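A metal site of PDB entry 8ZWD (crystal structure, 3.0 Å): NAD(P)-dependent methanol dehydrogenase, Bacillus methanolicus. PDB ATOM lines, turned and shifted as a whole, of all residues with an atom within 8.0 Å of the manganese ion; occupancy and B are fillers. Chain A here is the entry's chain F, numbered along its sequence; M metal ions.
NE2 of His 262 sits close to NE2 of His 276.
A ring nitrogen (ND1) of His 262 lies close to the side-chain hydroxyl of Ser 196, 3.4 Å away.
A ring nitrogen (ND1) of His 266 sits close to the backbone carbonyl oxygen (O) of His 262, at 3.2 Å.
OE1 of Glu 200 lies within hydrogen-bond range of ND1 of His 262, at 3.1 Å.
ND2 of Asn 280 lies close to OD1 of Asp 193 (2.9 Å).
The backbone carbonyl oxygen (O) of His 276 lies within hydrogen-bond range of the side-chain amide nitrogen (ND2) of Asn 280, at 3.2 Å.
His 276 touches the manganese ion.
The manganese ion is bound by NE2 of His 262 (2.0 Å), NE2 of His 197 (2.2 Å), OD2 of Asp 193 (2.5 Å) and OD1 of Asp 193 (2.6 Å).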
ATOM      1  N   GLY A 140      18.868 -14.613   4.433  1.00  0.00           N
ATOM      2  CA  GLY A 140      19.393 -15.513   3.429  1.00  0.00           C
ATOM      3  C   GLY A 140      19.514 -16.885   4.047  1.00  0.00           C
ATOM      4  O   GLY A 140      18.906 -17.180   5.083  1.00  0.00           O
ATOM      5  N   THR A 141      20.340 -17.740   3.422  1.00  0.00           N
ATOM      6  CA  THR A 141      20.622 -19.103   3.903  1.00  0.00           C
ATOM      7  C   THR A 141      19.347 -19.943   3.972  1.00  0.00           C
ATOM      8  O   THR A 141      19.280 -21.013   3.355  1.00  0.00           O
ATOM      9  CB  THR A 141      21.323 -19.102   5.276  1.00  0.00           C
ATOM     10  OG1 THR A 141      20.372 -18.922   6.343  1.00  0.00           O
ATOM     11  CG2 THR A 141      22.388 -18.009   5.370  1.00  0.00           C
ATOM     12  N   GLY A 142      18.351 -19.484   4.730  1.00  0.00           N
ATOM     13  CA  GLY A 142      17.163 -20.273   5.007  1.00  0.00           C
ATOM     14  C   GLY A 142      17.434 -21.501   5.827  1.00  0.00           C
ATOM     15  O   GLY A 142      16.546 -22.338   5.988  1.00  0.00           O
ATOM     16  N   SER A 143      18.653 -21.633   6.371  1.00  0.00           N
ATOM     17  CA  SER A 143      19.079 -22.842   7.067  1.00  0.00           C
ATOM     18  C   SER A 143      18.239 -23.141   8.292  1.00  0.00           C
ATOM     19  O   SER A 143      18.349 -24.238   8.850  1.00  0.00           O
ATOM     20  CB  SER A 143      20.546 -22.724   7.465  1.00  0.00           C
ATOM     21  OG  SER A 143      21.295 -22.182   6.383  1.00  0.00           O
ATOM     22  N   LEU A 148      20.083 -29.467   5.473  1.00  0.00           N
ATOM     23  CA  LEU A 148      21.446 -29.377   4.983  1.00  0.00           C
ATOM     24  C   LEU A 148      22.332 -28.580   5.922  1.00  0.00           C
ATOM     25  O   LEU A 148      21.865 -27.650   6.593  1.00  0.00           O
ATOM     26  CB  LEU A 148      21.463 -28.742   3.580  1.00  0.00           C
ATOM     27  CG  LEU A 148      22.798 -28.362   2.923  1.00  0.00           C
ATOM     28  CD1 LEU A 148      23.638 -29.585   2.620  1.00  0.00           C
ATOM     29  CD2 LEU A 148      22.548 -27.555   1.659  1.00  0.00           C
ATOM     30  N   VAL A 150      26.286 -26.895   5.531  1.00  0.00           N
ATOM     31  CA  VAL A 150      27.411 -26.665   4.630  1.00  0.00           C
ATOM     32  C   VAL A 150      28.702 -26.493   5.432  1.00  0.00           C
ATOM     33  O   VAL A 150      29.144 -25.362   5.682  1.00  0.00           O
ATOM     34  CB  VAL A 150      27.174 -25.442   3.722  1.00  0.00           C
ATOM     35  CG1 VAL A 150      28.255 -25.368   2.650  1.00  0.00           C
ATOM     36  CG2 VAL A 150      25.794 -25.554   3.055  1.00  0.00           C
ATOM     37  N   ALA A 189      24.513  -9.773   0.084  1.00  0.00           N
ATOM     38  CA  ALA A 189      24.955 -11.168   0.003  1.00  0.00           C
ATOM     39  C   ALA A 189      23.833 -12.124   0.389  1.00  0.00           C
ATOM     40  O   ALA A 189      23.494 -13.047  -0.379  1.00  0.00           O
ATOM     41  CB  ALA A 189      26.185 -11.374   0.893  1.00  0.00           C
ATOM     42  N   THR A 190      23.201 -11.908   1.544  1.00  0.00           N
ATOM     43  CA  THR A 190      22.152 -12.803   1.998  1.00  0.00           C
ATOM     44  C   THR A 190      20.949 -12.770   1.058  1.00  0.00           C
ATOM     45  O   THR A 190      20.397 -13.816   0.695  1.00  0.00           O
ATOM     46  CB  THR A 190      21.734 -12.452   3.426  1.00  0.00           C
ATOM     47  OG1 THR A 190      21.525 -11.040   3.534  1.00  0.00           O
ATOM     48  CG2 THR A 190      22.813 -12.879   4.409  1.00  0.00           C
ATOM     49  N   MET A 192      20.741 -11.858  -2.161  1.00  0.00           N
ATOM     50  CA  MET A 192      21.054 -12.452  -3.454  1.00  0.00           C
ATOM     51  C   MET A 192      21.174 -13.956  -3.357  1.00  0.00           C
ATOM     52  O   MET A 192      20.795 -14.656  -4.300  1.00  0.00           O
ATOM     53  CB  MET A 192      22.329 -11.838  -4.017  1.00  0.00           C
ATOM     54  CG  MET A 192      22.098 -10.496  -4.652  1.00  0.00           C
ATOM     55  SD  MET A 192      20.793 -10.583  -5.890  1.00  0.00           S
ATOM     56  CE  MET A 192      21.574 -11.554  -7.180  1.00  0.00           C
ATOM     57  N   ASP A 193      21.669 -14.483  -2.224  1.00  0.00           N
ATOM     58  CA  ASP A 193      21.632 -15.935  -2.073  1.00  0.00           C
ATOM     59  C   ASP A 193      20.195 -16.445  -1.981  1.00  0.00           C
ATOM     60  O   ASP A 193      19.887 -17.525  -2.501  1.00  0.00           O
ATOM     61  CB  ASP A 193      22.432 -16.383  -0.854  1.00  0.00           C
ATOM     62  CG  ASP A 193      22.729 -17.885  -0.856  1.00  0.00           C
ATOM     63  OD1 ASP A 193      22.736 -18.512  -1.942  1.00  0.00           O
ATOM     64  OD2 ASP A 193      22.937 -18.441   0.247  1.00  0.00           O
ATOM     65  N   ALA A 194      19.304 -15.705  -1.332  1.00  0.00           N
ATOM     66  CA  ALA A 194      17.900 -16.131  -1.295  1.00  0.00           C
ATOM     67  C   ALA A 194      17.305 -16.147  -2.697  1.00  0.00           C
ATOM     68  O   ALA A 194      16.566 -17.069  -3.063  1.00  0.00           O
ATOM     69  CB  ALA A 194      17.107 -15.227  -0.361  1.00  0.00           C
ATOM     70  N   SER A 196      19.018 -16.667  -5.347  1.00  0.00           N
ATOM     71  CA  SER A 196      19.645 -17.866  -5.879  1.00  0.00           C
ATOM     72  C   SER A 196      18.831 -19.115  -5.534  1.00  0.00           C
ATOM     73  O   SER A 196      18.586 -19.971  -6.399  1.00  0.00           O
ATOM     74  CB  SER A 196      21.064 -17.971  -5.331  1.00  0.00           C
ATOM     75  OG  SER A 196      21.595 -19.279  -5.506  1.00  0.00           O
ATOM     76  N   HIS A 197      18.423 -19.236  -4.280  1.00  0.00           N
ATOM     77  CA  HIS A 197      17.685 -20.416  -3.855  1.00  0.00           C
ATOM     78  C   HIS A 197      16.378 -20.528  -4.626  1.00  0.00           C
ATOM     79  O   HIS A 197      16.049 -21.592  -5.160  1.00  0.00           O
ATOM     80  CB  HIS A 197      17.441 -20.371  -2.347  1.00  0.00           C
ATOM     81  CG  HIS A 197      18.691 -20.419  -1.529  1.00  0.00           C
ATOM     82  ND1 HIS A 197      18.741 -20.044  -0.203  1.00  0.00           N
ATOM     83  CD2 HIS A 197      19.952 -20.791  -1.856  1.00  0.00           C
ATOM     84  CE1 HIS A 197      19.973 -20.189   0.255  1.00  0.00           C
ATOM     85  NE2 HIS A 197      20.724 -20.640  -0.728  1.00  0.00           N
ATOM     86  N   GLU A 200      17.143 -21.477  -8.468  1.00  0.00           N
ATOM     87  CA  GLU A 200      17.594 -22.854  -8.629  1.00  0.00           C
ATOM     88  C   GLU A 200      16.477 -23.849  -8.353  1.00  0.00           C
ATOM     89  O   GLU A 200      16.307 -24.812  -9.112  1.00  0.00           O
ATOM     90  CB  GLU A 200      18.798 -23.120  -7.714  1.00  0.00           C
ATOM     91  CG  GLU A 200      20.020 -22.233  -8.002  1.00  0.00           C
ATOM     92  CD  GLU A 200      21.284 -23.047  -8.231  1.00  0.00           C
ATOM     93  OE1 GLU A 200      21.989 -23.369  -7.244  1.00  0.00           O
ATOM     94  OE2 GLU A 200      21.579 -23.356  -9.408  1.00  0.00           O
ATOM     95  N   PHE A 253      14.401 -24.924  -1.838  1.00  0.00           N
ATOM     96  CA  PHE A 253      15.604 -25.621  -2.275  1.00  0.00           C
ATOM     97  C   PHE A 253      15.880 -26.854  -1.425  1.00  0.00           C
ATOM     98  O   PHE A 253      16.453 -27.821  -1.935  1.00  0.00           O
ATOM     99  CB  PHE A 253      16.820 -24.672  -2.308  1.00  0.00           C
ATOM    100  CG  PHE A 253      17.587 -24.551  -1.010  1.00  0.00           C
ATOM    101  CD1 PHE A 253      18.440 -25.547  -0.575  1.00  0.00           C
ATOM    102  CD2 PHE A 253      17.506 -23.379  -0.272  1.00  0.00           C
ATOM    103  CE1 PHE A 253      19.145 -25.411   0.601  1.00  0.00           C
ATOM    104  CE2 PHE A 253      18.214 -23.233   0.906  1.00  0.00           C
ATOM    105  CZ  PHE A 253      19.042 -24.256   1.340  1.00  0.00           C
ATOM    106  N   LEU A 258      18.897 -27.692  -5.854  1.00  0.00           N
ATOM    107  CA  LEU A 258      19.546 -26.486  -6.281  1.00  0.00           C
ATOM    108  C   LEU A 258      20.173 -26.686  -7.648  1.00  0.00           C
ATOM    109  O   LEU A 258      19.498 -27.028  -8.594  1.00  0.00           O
ATOM    110  CB  LEU A 258      20.595 -26.073  -5.261  1.00  0.00           C
ATOM    111  CG  LEU A 258      20.194 -25.383  -3.961  1.00  0.00           C
ATOM    112  CD1 LEU A 258      21.315 -25.503  -2.949  1.00  0.00           C
ATOM    113  CD2 LEU A 258      19.874 -23.928  -4.218  1.00  0.00           C
ATOM    114  N   VAL A 261      24.872 -23.256  -9.690  1.00  0.00           N
ATOM    115  CA  VAL A 261      25.247 -22.015  -8.994  1.00  0.00           C
ATOM    116  C   VAL A 261      25.947 -22.354  -7.682  1.00  0.00           C
ATOM    117  O   VAL A 261      27.103 -21.966  -7.461  1.00  0.00           O
ATOM    118  CB  VAL A 261      24.014 -21.124  -8.770  1.00  0.00           C
ATOM    119  CG1 VAL A 261      24.372 -19.896  -7.930  1.00  0.00           C
ATOM    120  CG2 VAL A 261      23.415 -20.709 -10.098  1.00  0.00           C
ATOM    121  N   HIS A 262      25.266 -23.087  -6.802  1.00  0.00           N
ATOM    122  CA  HIS A 262      25.857 -23.424  -5.523  1.00  0.00           C
ATOM    123  C   HIS A 262      27.032 -24.386  -5.667  1.00  0.00           C
ATOM    124  O   HIS A 262      27.997 -24.297  -4.896  1.00  0.00           O
ATOM    125  CB  HIS A 262      24.801 -23.987  -4.589  1.00  0.00           C
ATOM    126  CG  HIS A 262      24.010 -22.923  -3.888  1.00  0.00           C
ATOM    127  ND1 HIS A 262      22.995 -22.224  -4.514  1.00  0.00           N
ATOM    128  CD2 HIS A 262      24.087 -22.423  -2.629  1.00  0.00           C
ATOM    129  CE1 HIS A 262      22.479 -21.347  -3.669  1.00  0.00           C
ATOM    130  NE2 HIS A 262      23.135 -21.444  -2.518  1.00  0.00           N
ATOM    131  N   SER A 265      29.914 -21.976  -6.568  1.00  0.00           N
ATOM    132  CA  SER A 265      30.288 -21.043  -5.508  1.00  0.00           C
ATOM    133  C   SER A 265      30.831 -21.763  -4.288  1.00  0.00           C
ATOM    134  O   SER A 265      31.653 -21.194  -3.568  1.00  0.00           O
ATOM    135  CB  SER A 265      29.101 -20.168  -5.130  1.00  0.00           C
ATOM    136  OG  SER A 265      28.633 -19.462  -6.261  1.00  0.00           O
ATOM    137  N   HIS A 266      30.428 -23.019  -4.051  1.00  0.00           N
ATOM    138  CA  HIS A 266      31.017 -23.774  -2.946  1.00  0.00           C
ATOM    139  C   HIS A 266      32.513 -23.869  -3.115  1.00  0.00           C
ATOM    140  O   HIS A 266      33.277 -23.601  -2.184  1.00  0.00           O
ATOM    141  CB  HIS A 266      30.408 -25.169  -2.880  1.00  0.00           C
ATOM    142  CG  HIS A 266      29.056 -25.215  -2.253  1.00  0.00           C
ATOM    143  ND1 HIS A 266      28.190 -26.285  -2.396  1.00  0.00           N
ATOM    144  CD2 HIS A 266      28.408 -24.319  -1.466  1.00  0.00           C
ATOM    145  CE1 HIS A 266      27.074 -26.039  -1.732  1.00  0.00           C
ATOM    146  NE2 HIS A 266      27.181 -24.860  -1.156  1.00  0.00           N
ATOM    147  N   HIS A 276      29.382 -15.993   0.044  1.00  0.00           N
ATOM    148  CA  HIS A 276      28.570 -16.938  -0.703  1.00  0.00           C
ATOM    149  C   HIS A 276      27.664 -16.233  -1.704  1.00  0.00           C
ATOM    150  O   HIS A 276      27.678 -16.542  -2.897  1.00  0.00           O
ATOM    151  CB  HIS A 276      27.737 -17.769   0.269  1.00  0.00           C
ATOM    152  CG  HIS A 276      27.142 -18.991  -0.359  1.00  0.00           C
ATOM    153  ND1 HIS A 276      27.849 -19.784  -1.242  1.00  0.00           N
ATOM    154  CD2 HIS A 276      25.917 -19.561  -0.238  1.00  0.00           C
ATOM    155  CE1 HIS A 276      27.083 -20.780  -1.635  1.00  0.00           C
ATOM    156  NE2 HIS A 276      25.912 -20.669  -1.044  1.00  0.00           N
ATOM    157  N   GLY A 277      26.832 -15.310  -1.221  1.00  0.00           N
ATOM    158  CA  GLY A 277      25.901 -14.635  -2.099  1.00  0.00           C
ATOM    159  C   GLY A 277      26.582 -13.883  -3.222  1.00  0.00           C
ATOM    160  O   GLY A 277      26.061 -13.823  -4.338  1.00  0.00           O
ATOM    161  N   ASN A 280      27.647 -16.420  -5.841  1.00  0.00           N
ATOM    162  CA  ASN A 280      26.444 -16.919  -6.512  1.00  0.00           C
ATOM    163  C   ASN A 280      25.930 -15.912  -7.520  1.00  0.00           C
ATOM    164  O   ASN A 280      25.597 -16.281  -8.657  1.00  0.00           O
ATOM    165  CB  ASN A 280      25.360 -17.233  -5.485  1.00  0.00           C
ATOM    166  CG  ASN A 280      25.615 -18.514  -4.711  1.00  0.00           C
ATOM    167  OD1 ASN A 280      26.120 -19.486  -5.252  1.00  0.00           O
ATOM    168  ND2 ASN A 280      25.250 -18.511  -3.436  1.00  0.00           N
HETATM  169 MN    MN M   1      22.952 -20.725  -0.665  1.00  0.00          MN
